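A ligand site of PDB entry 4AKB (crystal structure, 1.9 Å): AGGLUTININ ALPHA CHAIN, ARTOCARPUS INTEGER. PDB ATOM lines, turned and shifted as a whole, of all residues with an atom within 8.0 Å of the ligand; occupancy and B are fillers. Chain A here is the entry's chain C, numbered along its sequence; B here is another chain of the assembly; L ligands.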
ATOM      1  N   GLY A   1      -1.278  -9.203 -28.924  1.00  0.00           N
ATOM      2  CA  GLY A   1      -0.095  -9.944 -29.349  1.00  0.00           C
ATOM      3  C   GLY A   1      -0.334 -11.435 -29.470  1.00  0.00           C
ATOM      4  O   GLY A   1      -1.445 -11.917 -29.212  1.00  0.00           O
ATOM      5  N   LYS A   2       0.726 -12.191 -29.853  1.00  0.00           N
ATOM      6  CA  LYS A   2       0.677 -13.642 -30.011  1.00  0.00           C
ATOM      7  C   LYS A   2       0.905 -14.338 -28.667  1.00  0.00           C
ATOM      8  O   LYS A   2       1.999 -14.256 -28.111  1.00  0.00           O
ATOM      9  CB  LYS A   2       1.733 -14.100 -31.045  1.00  0.00           C
ATOM     10  CG  LYS A   2       1.639 -15.584 -31.421  1.00  0.00           C
ATOM     11  CD  LYS A   2       2.959 -16.098 -31.988  1.00  0.00           C
ATOM     12  CE  LYS A   2       2.780 -17.422 -32.688  1.00  0.00           C
ATOM     13  NZ  LYS A   2       4.064 -17.928 -33.263  1.00  0.00           N
ATOM     14  N   ALA A  24      10.055  -1.340 -23.501  1.00  0.00           N
ATOM     15  CA  ALA A  24       9.732  -2.503 -22.681  1.00  0.00           C
ATOM     16  C   ALA A  24      10.525  -3.753 -23.099  1.00  0.00           C
ATOM     17  O   ALA A  24      11.442  -3.672 -23.921  1.00  0.00           O
ATOM     18  CB  ALA A  24       8.241  -2.779 -22.770  1.00  0.00           C
ATOM     19  N   ILE A  25      10.158  -4.917 -22.490  1.00  0.00           N
ATOM     20  CA  ILE A  25      10.733  -6.234 -22.770  1.00  0.00           C
ATOM     21  C   ILE A  25      10.215  -6.665 -24.138  1.00  0.00           C
ATOM     22  O   ILE A  25       9.040  -6.464 -24.441  1.00  0.00           O
ATOM     23  CB  ILE A  25      10.311  -7.262 -21.666  1.00  0.00           C
ATOM     24  CG1 ILE A  25      10.839  -6.881 -20.247  1.00  0.00           C
ATOM     25  CG2 ILE A  25      10.683  -8.729 -22.061  1.00  0.00           C
ATOM     26  CD1 ILE A  25      12.451  -6.954 -19.998  1.00  0.00           C
ATOM     27  N   SER A  46       9.299 -10.709 -30.565  1.00  0.00           N
ATOM     28  CA  SER A  46       8.584  -9.451 -30.736  1.00  0.00           C
ATOM     29  C   SER A  46       8.302  -9.271 -32.231  1.00  0.00           C
ATOM     30  O   SER A  46       9.053  -9.769 -33.061  1.00  0.00           O
ATOM     31  CB  SER A  46       9.443  -8.285 -30.265  1.00  0.00           C
ATOM     32  OG  SER A  46       8.988  -7.048 -30.790  1.00  0.00           O
ATOM     33  N   PHE A  47       7.248  -8.520 -32.552  1.00  0.00           N
ATOM     34  CA  PHE A  47       6.889  -8.192 -33.940  1.00  0.00           C
ATOM     35  C   PHE A  47       7.855  -7.145 -34.517  1.00  0.00           C
ATOM     36  O   PHE A  47       7.854  -6.910 -35.725  1.00  0.00           O
ATOM     37  CB  PHE A  47       5.433  -7.708 -34.047  1.00  0.00           C
ATOM     38  CG  PHE A  47       4.315  -8.627 -33.577  1.00  0.00           C
ATOM     39  CD1 PHE A  47       4.521 -10.000 -33.441  1.00  0.00           C
ATOM     40  CD2 PHE A  47       3.029  -8.128 -33.338  1.00  0.00           C
ATOM     41  CE1 PHE A  47       3.489 -10.837 -33.013  1.00  0.00           C
ATOM     42  CE2 PHE A  47       1.999  -8.972 -32.925  1.00  0.00           C
ATOM     43  CZ  PHE A  47       2.238 -10.328 -32.755  1.00  0.00           C
ATOM     44  N   ILE A  48       8.677  -6.509 -33.652  1.00  0.00           N
ATOM     45  CA  ILE A  48       9.647  -5.463 -34.053  1.00  0.00           C
ATOM     46  C   ILE A  48      11.092  -5.792 -33.609  1.00  0.00           C
ATOM     47  O   ILE A  48      11.307  -6.746 -32.876  1.00  0.00           O
ATOM     48  CB  ILE A  48       9.198  -4.040 -33.599  1.00  0.00           C
ATOM     49  CG1 ILE A  48       8.941  -3.956 -32.075  1.00  0.00           C
ATOM     50  CG2 ILE A  48       7.998  -3.531 -34.411  1.00  0.00           C
ATOM     51  CD1 ILE A  48       9.493  -2.685 -31.402  1.00  0.00           C
ATOM     52  N   VAL A  75       3.062   1.706 -22.911  1.00  0.00           N
ATOM     53  CA  VAL A  75       4.015   1.980 -23.994  1.00  0.00           C
ATOM     54  C   VAL A  75       3.141   2.042 -25.238  1.00  0.00           C
ATOM     55  O   VAL A  75       2.473   1.056 -25.563  1.00  0.00           O
ATOM     56  CB  VAL A  75       5.179   0.960 -24.140  1.00  0.00           C
ATOM     57  CG1 VAL A  75       6.158   1.398 -25.223  1.00  0.00           C
ATOM     58  CG2 VAL A  75       5.932   0.764 -22.826  1.00  0.00           C
ATOM     59  N   SER A  76       3.072   3.233 -25.885  1.00  0.00           N
ATOM     60  CA  SER A  76       2.261   3.524 -27.070  1.00  0.00           C
ATOM     61  C   SER A  76       0.757   3.195 -26.888  1.00  0.00           C
ATOM     62  O   SER A  76       0.068   2.868 -27.861  1.00  0.00           O
ATOM     63  CB  SER A  76       2.844   2.862 -28.317  1.00  0.00           C
ATOM     64  OG  SER A  76       4.158   3.342 -28.582  1.00  0.00           O
ATOM     65  N   GLY A  77       0.282   3.309 -25.646  1.00  0.00           N
ATOM     66  CA  GLY A  77      -1.109   3.048 -25.272  1.00  0.00           C
ATOM     67  C   GLY A  77      -1.396   1.639 -24.800  1.00  0.00           C
ATOM     68  O   GLY A  77      -2.474   1.380 -24.251  1.00  0.00           O
ATOM     69  N   TYR A  78      -0.432   0.710 -24.988  1.00  0.00           N
ATOM     70  CA  TYR A  78      -0.581  -0.684 -24.574  1.00  0.00           C
ATOM     71  C   TYR A  78      -0.057  -0.930 -23.180  1.00  0.00           C
ATOM     72  O   TYR A  78       0.999  -0.398 -22.814  1.00  0.00           O
ATOM     73  CB  TYR A  78       0.135  -1.620 -25.565  1.00  0.00           C
ATOM     74  CG  TYR A  78      -0.419  -1.567 -26.973  1.00  0.00           C
ATOM     75  CD1 TYR A  78      -1.567  -2.253 -27.314  1.00  0.00           C
ATOM     76  CD2 TYR A  78       0.242  -0.843 -27.965  1.00  0.00           C
ATOM     77  CE1 TYR A  78      -2.075  -2.217 -28.616  1.00  0.00           C
ATOM     78  CE2 TYR A  78      -0.249  -0.813 -29.275  1.00  0.00           C
ATOM     79  CZ  TYR A  78      -1.400  -1.506 -29.594  1.00  0.00           C
ATOM     80  OH  TYR A  78      -1.887  -1.497 -30.883  1.00  0.00           O
ATOM     81  N   VAL A  79      -0.760  -1.761 -22.401  1.00  0.00           N
ATOM     82  CA  VAL A  79      -0.289  -2.156 -21.073  1.00  0.00           C
ATOM     83  C   VAL A  79       0.632  -3.357 -21.326  1.00  0.00           C
ATOM     84  O   VAL A  79       0.206  -4.361 -21.902  1.00  0.00           O
ATOM     85  CB  VAL A  79      -1.437  -2.474 -20.084  1.00  0.00           C
ATOM     86  CG1 VAL A  79      -0.895  -3.047 -18.781  1.00  0.00           C
ATOM     87  CG2 VAL A  79      -2.288  -1.220 -19.812  1.00  0.00           C
ATOM     88  N   VAL A  80       1.926  -3.215 -20.988  1.00  0.00           N
ATOM     89  CA  VAL A  80       2.953  -4.240 -21.249  1.00  0.00           C
ATOM     90  C   VAL A  80       3.863  -4.413 -20.006  1.00  0.00           C
ATOM     91  O   VAL A  80       3.724  -3.671 -19.031  1.00  0.00           O
ATOM     92  CB  VAL A  80       3.801  -3.879 -22.511  1.00  0.00           C
ATOM     93  CG1 VAL A  80       2.954  -3.813 -23.797  1.00  0.00           C
ATOM     94  CG2 VAL A  80       4.581  -2.575 -22.318  1.00  0.00           C
ATOM     95  N   VAL A  81       4.809  -5.388 -20.059  1.00  0.00           N
ATOM     96  CA  VAL A  81       5.810  -5.652 -19.025  1.00  0.00           C
ATOM     97  C   VAL A  81       7.037  -4.834 -19.466  1.00  0.00           C
ATOM     98  O   VAL A  81       7.625  -5.120 -20.507  1.00  0.00           O
ATOM     99  CB  VAL A  81       6.092  -7.174 -18.877  1.00  0.00           C
ATOM    100  CG1 VAL A  81       7.112  -7.439 -17.778  1.00  0.00           C
ATOM    101  CG2 VAL A  81       4.809  -7.945 -18.605  1.00  0.00           C
ATOM    102  N   SER A 119       2.110 -13.500 -23.569  1.00  0.00           N
ATOM    103  CA  SER A 119       1.813 -12.974 -24.904  1.00  0.00           C
ATOM    104  C   SER A 119       2.785 -11.895 -25.274  1.00  0.00           C
ATOM    105  O   SER A 119       3.187 -11.108 -24.420  1.00  0.00           O
ATOM    106  CB  SER A 119       0.388 -12.417 -24.967  1.00  0.00           C
ATOM    107  OG  SER A 119       0.138 -11.815 -26.227  1.00  0.00           O
ATOM    108  N   ILE A 120       3.157 -11.843 -26.570  1.00  0.00           N
ATOM    109  CA  ILE A 120       4.092 -10.839 -27.089  1.00  0.00           C
ATOM    110  C   ILE A 120       3.574 -10.286 -28.399  1.00  0.00           C
ATOM    111  O   ILE A 120       3.223 -11.071 -29.292  1.00  0.00           O
ATOM    112  CB  ILE A 120       5.546 -11.420 -27.238  1.00  0.00           C
ATOM    113  CG1 ILE A 120       6.066 -12.041 -25.907  1.00  0.00           C
ATOM    114  CG2 ILE A 120       6.529 -10.350 -27.747  1.00  0.00           C
ATOM    115  CD1 ILE A 120       7.437 -12.708 -26.006  1.00  0.00           C
ATOM    116  N   GLY A 121       3.557  -8.963 -28.492  1.00  0.00           N
ATOM    117  CA  GLY A 121       3.201  -8.223 -29.700  1.00  0.00           C
ATOM    118  C   GLY A 121       4.448  -7.475 -30.080  1.00  0.00           C
ATOM    119  O   GLY A 121       5.462  -8.092 -30.430  1.00  0.00           O
ATOM    120  N   TYR A 122       4.424  -6.135 -29.911  1.00  0.00           N
ATOM    121  CA  TYR A 122       5.615  -5.304 -30.074  1.00  0.00           C
ATOM    122  C   TYR A 122       6.464  -5.581 -28.822  1.00  0.00           C
ATOM    123  O   TYR A 122       7.683  -5.688 -28.895  1.00  0.00           O
ATOM    124  CB  TYR A 122       5.248  -3.801 -30.100  1.00  0.00           C
ATOM    125  CG  TYR A 122       4.421  -3.319 -31.268  1.00  0.00           C
ATOM    126  CD1 TYR A 122       4.731  -3.697 -32.569  1.00  0.00           C
ATOM    127  CD2 TYR A 122       3.414  -2.366 -31.090  1.00  0.00           C
ATOM    128  CE1 TYR A 122       3.995  -3.219 -33.662  1.00  0.00           C
ATOM    129  CE2 TYR A 122       2.676  -1.881 -32.167  1.00  0.00           C
ATOM    130  CZ  TYR A 122       2.969  -2.304 -33.452  1.00  0.00           C
ATOM    131  OH  TYR A 122       2.249  -1.805 -34.526  1.00  0.00           O
ATOM    132  N   TRP A 123       5.781  -5.771 -27.659  1.00  0.00           N
ATOM    133  CA  TRP A 123       6.406  -6.015 -26.366  1.00  0.00           C
ATOM    134  C   TRP A 123       5.713  -7.162 -25.635  1.00  0.00           C
ATOM    135  O   TRP A 123       4.644  -7.607 -26.056  1.00  0.00           O
ATOM    136  CB  TRP A 123       6.395  -4.699 -25.529  1.00  0.00           C
ATOM    137  CG  TRP A 123       7.038  -3.542 -26.251  1.00  0.00           C
ATOM    138  CD1 TRP A 123       8.363  -3.417 -26.561  1.00  0.00           C
ATOM    139  CD2 TRP A 123       6.375  -2.447 -26.907  1.00  0.00           C
ATOM    140  NE1 TRP A 123       8.571  -2.283 -27.314  1.00  0.00           N
ATOM    141  CE2 TRP A 123       7.366  -1.686 -27.567  1.00  0.00           C
ATOM    142  CE3 TRP A 123       5.036  -2.029 -26.992  1.00  0.00           C
ATOM    143  CZ2 TRP A 123       7.064  -0.524 -28.299  1.00  0.00           C
ATOM    144  CZ3 TRP A 123       4.726  -0.884 -27.731  1.00  0.00           C
ATOM    145  CH2 TRP A 123       5.742  -0.143 -28.374  1.00  0.00           C
ATOM    146  N   LEU A 124       6.362  -7.674 -24.557  1.00  0.00           N
ATOM    147  CA  LEU A 124       5.803  -8.709 -23.710  1.00  0.00           C
ATOM    148  C   LEU A 124       4.586  -8.084 -23.044  1.00  0.00           C
ATOM    149  O   LEU A 124       4.737  -7.131 -22.268  1.00  0.00           O
ATOM    150  CB  LEU A 124       6.853  -9.166 -22.669  1.00  0.00           C
ATOM    151  CG  LEU A 124       6.429 -10.158 -21.592  1.00  0.00           C
ATOM    152  CD1 LEU A 124       5.970 -11.473 -22.210  1.00  0.00           C
ATOM    153  CD2 LEU A 124       7.571 -10.397 -20.588  1.00  0.00           C
ATOM    154  N   ASP A 125       3.367  -8.521 -23.449  1.00  0.00           N
ATOM    155  CA  ASP A 125       2.106  -7.958 -22.956  1.00  0.00           C
ATOM    156  C   ASP A 125       1.854  -8.354 -21.509  1.00  0.00           C
ATOM    157  O   ASP A 125       1.503  -7.507 -20.682  1.00  0.00           O
ATOM    158  CB  ASP A 125       0.934  -8.406 -23.833  1.00  0.00           C
ATOM    159  CG  ASP A 125       1.123  -8.078 -25.298  1.00  0.00           C
ATOM    160  OD1 ASP A 125       1.357  -6.908 -25.613  1.00  0.00           O
ATOM    161  OD2 ASP A 125       1.100  -9.027 -26.123  1.00  0.00           O
ATOM    162  N   TYR A 126       2.029  -9.656 -21.217  1.00  0.00           N
ATOM    163  CA  TYR A 126       1.823 -10.242 -19.913  1.00  0.00           C
ATOM    164  C   TYR A 126       2.532 -11.584 -19.823  1.00  0.00           C
ATOM    165  O   TYR A 126       2.910 -12.156 -20.837  1.00  0.00           O
ATOM    166  CB  TYR A 126       0.308 -10.429 -19.602  1.00  0.00           C
ATOM    167  CG  TYR A 126      -0.446 -11.315 -20.578  1.00  0.00           C
ATOM    168  CD1 TYR A 126      -0.468 -12.696 -20.411  1.00  0.00           C
ATOM    169  CD2 TYR A 126      -1.180 -10.763 -21.620  1.00  0.00           C
ATOM    170  CE1 TYR A 126      -1.167 -13.519 -21.311  1.00  0.00           C
ATOM    171  CE2 TYR A 126      -1.910 -11.568 -22.500  1.00  0.00           C
ATOM    172  CZ  TYR A 126      -1.893 -12.951 -22.346  1.00  0.00           C
ATOM    173  OH  TYR A 126      -2.586 -13.752 -23.223  1.00  0.00           O
ATOM    174  N   ALA B  17      -0.735  -6.812 -19.266  1.00  0.00           N
ATOM    175  CA  ALA B  17      -2.053  -6.581 -19.887  1.00  0.00           C
ATOM    176  C   ALA B  17      -3.089  -7.638 -19.496  1.00  0.00           C
ATOM    177  O   ALA B  17      -2.715  -8.779 -19.201  1.00  0.00           O
ATOM    178  CB  ALA B  17      -1.929  -6.559 -21.395  1.00  0.00           C
HETATM  179  C1  LIG L   1       0.850  -4.933 -31.056  1.00  0.00           C
HETATM  180  C2  LIG L   1      -0.266  -5.962 -30.873  1.00  0.00           C
HETATM  181  C3  LIG L   1      -1.096  -5.599 -29.642  1.00  0.00           C
HETATM  182  C4  LIG L   1      -0.205  -5.475 -28.407  1.00  0.00           C
HETATM  183  C5  LIG L   1       0.922  -4.484 -28.686  1.00  0.00           C
HETATM  184  C6  LIG L   1       1.910  -4.297 -27.553  1.00  0.00           C
HETATM  185  O1  LIG L   1       1.625  -5.294 -32.138  1.00  0.00           O
HETATM  186  O2  LIG L   1      -1.100  -6.011 -32.037  1.00  0.00           O
HETATM  187  O3  LIG L   1      -2.123  -6.561 -29.438  1.00  0.00           O
HETATM  188  O4  LIG L   1       0.327  -6.751 -28.059  1.00  0.00           O
HETATM  189  O5  LIG L   1       1.656  -4.870 -29.863  1.00  0.00           O
HETATM  190  O6  LIG L   1       2.796  -5.403 -27.410  1.00  0.00           O
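O3 of the ligand sits at hydrogen-bond distance from N of Gly 1 (2.8 Å).
The backbone NH of Trp 123 is in hydrogen-bond range of an oxygen (O6) of the ligand (3.0 Å).
An oxygen (O5) of the ligand is in hydrogen-bond range of the backbone NH of Tyr 122.
The backbone carbonyl oxygen (O) of Trp 123 is in hydrogen-bond range of an oxygen (O6) of the ligand.
O4 of the ligand lies within hydrogen-bond range of OD1 of Asp 125 (2.7 Å).
Merely in contact with the ligand: Phe 47, Tyr 78, Gly 121 and Val 80.
Hydrophobic or aromatic side chains within 4 Å of the ligand: Phe 47, Tyr 78, Val 80, Tyr 122 and Trp 123.
The nearest printed residue that does not touch the ligand is Ile 120 (4.8 Å).
O of Asp 125 is in hydrogen-bond range of N of Ala 17 of chain B, 2.7 Å away.
The side-chain carboxylate (OD2) of Asp 125 lies within hydrogen-bond range of the backbone NH (N) of Gly 121 (3.4 Å).
The backbone carbonyl oxygen (O) of Tyr 122 sits at hydrogen-bond distance from the side-chain hydroxyl (OG) of Ser 46, 2.7 Å away.
N of Phe 47 lies within hydrogen-bond range of O of Gly 121.
The side-chain hydroxyl of Ser 119 lies close to the backbone carbonyl oxygen of Gly 1 (3.4 Å).
N of Asp 125 sits at hydrogen-bond distance from O of Ser 119 (2.8 Å).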
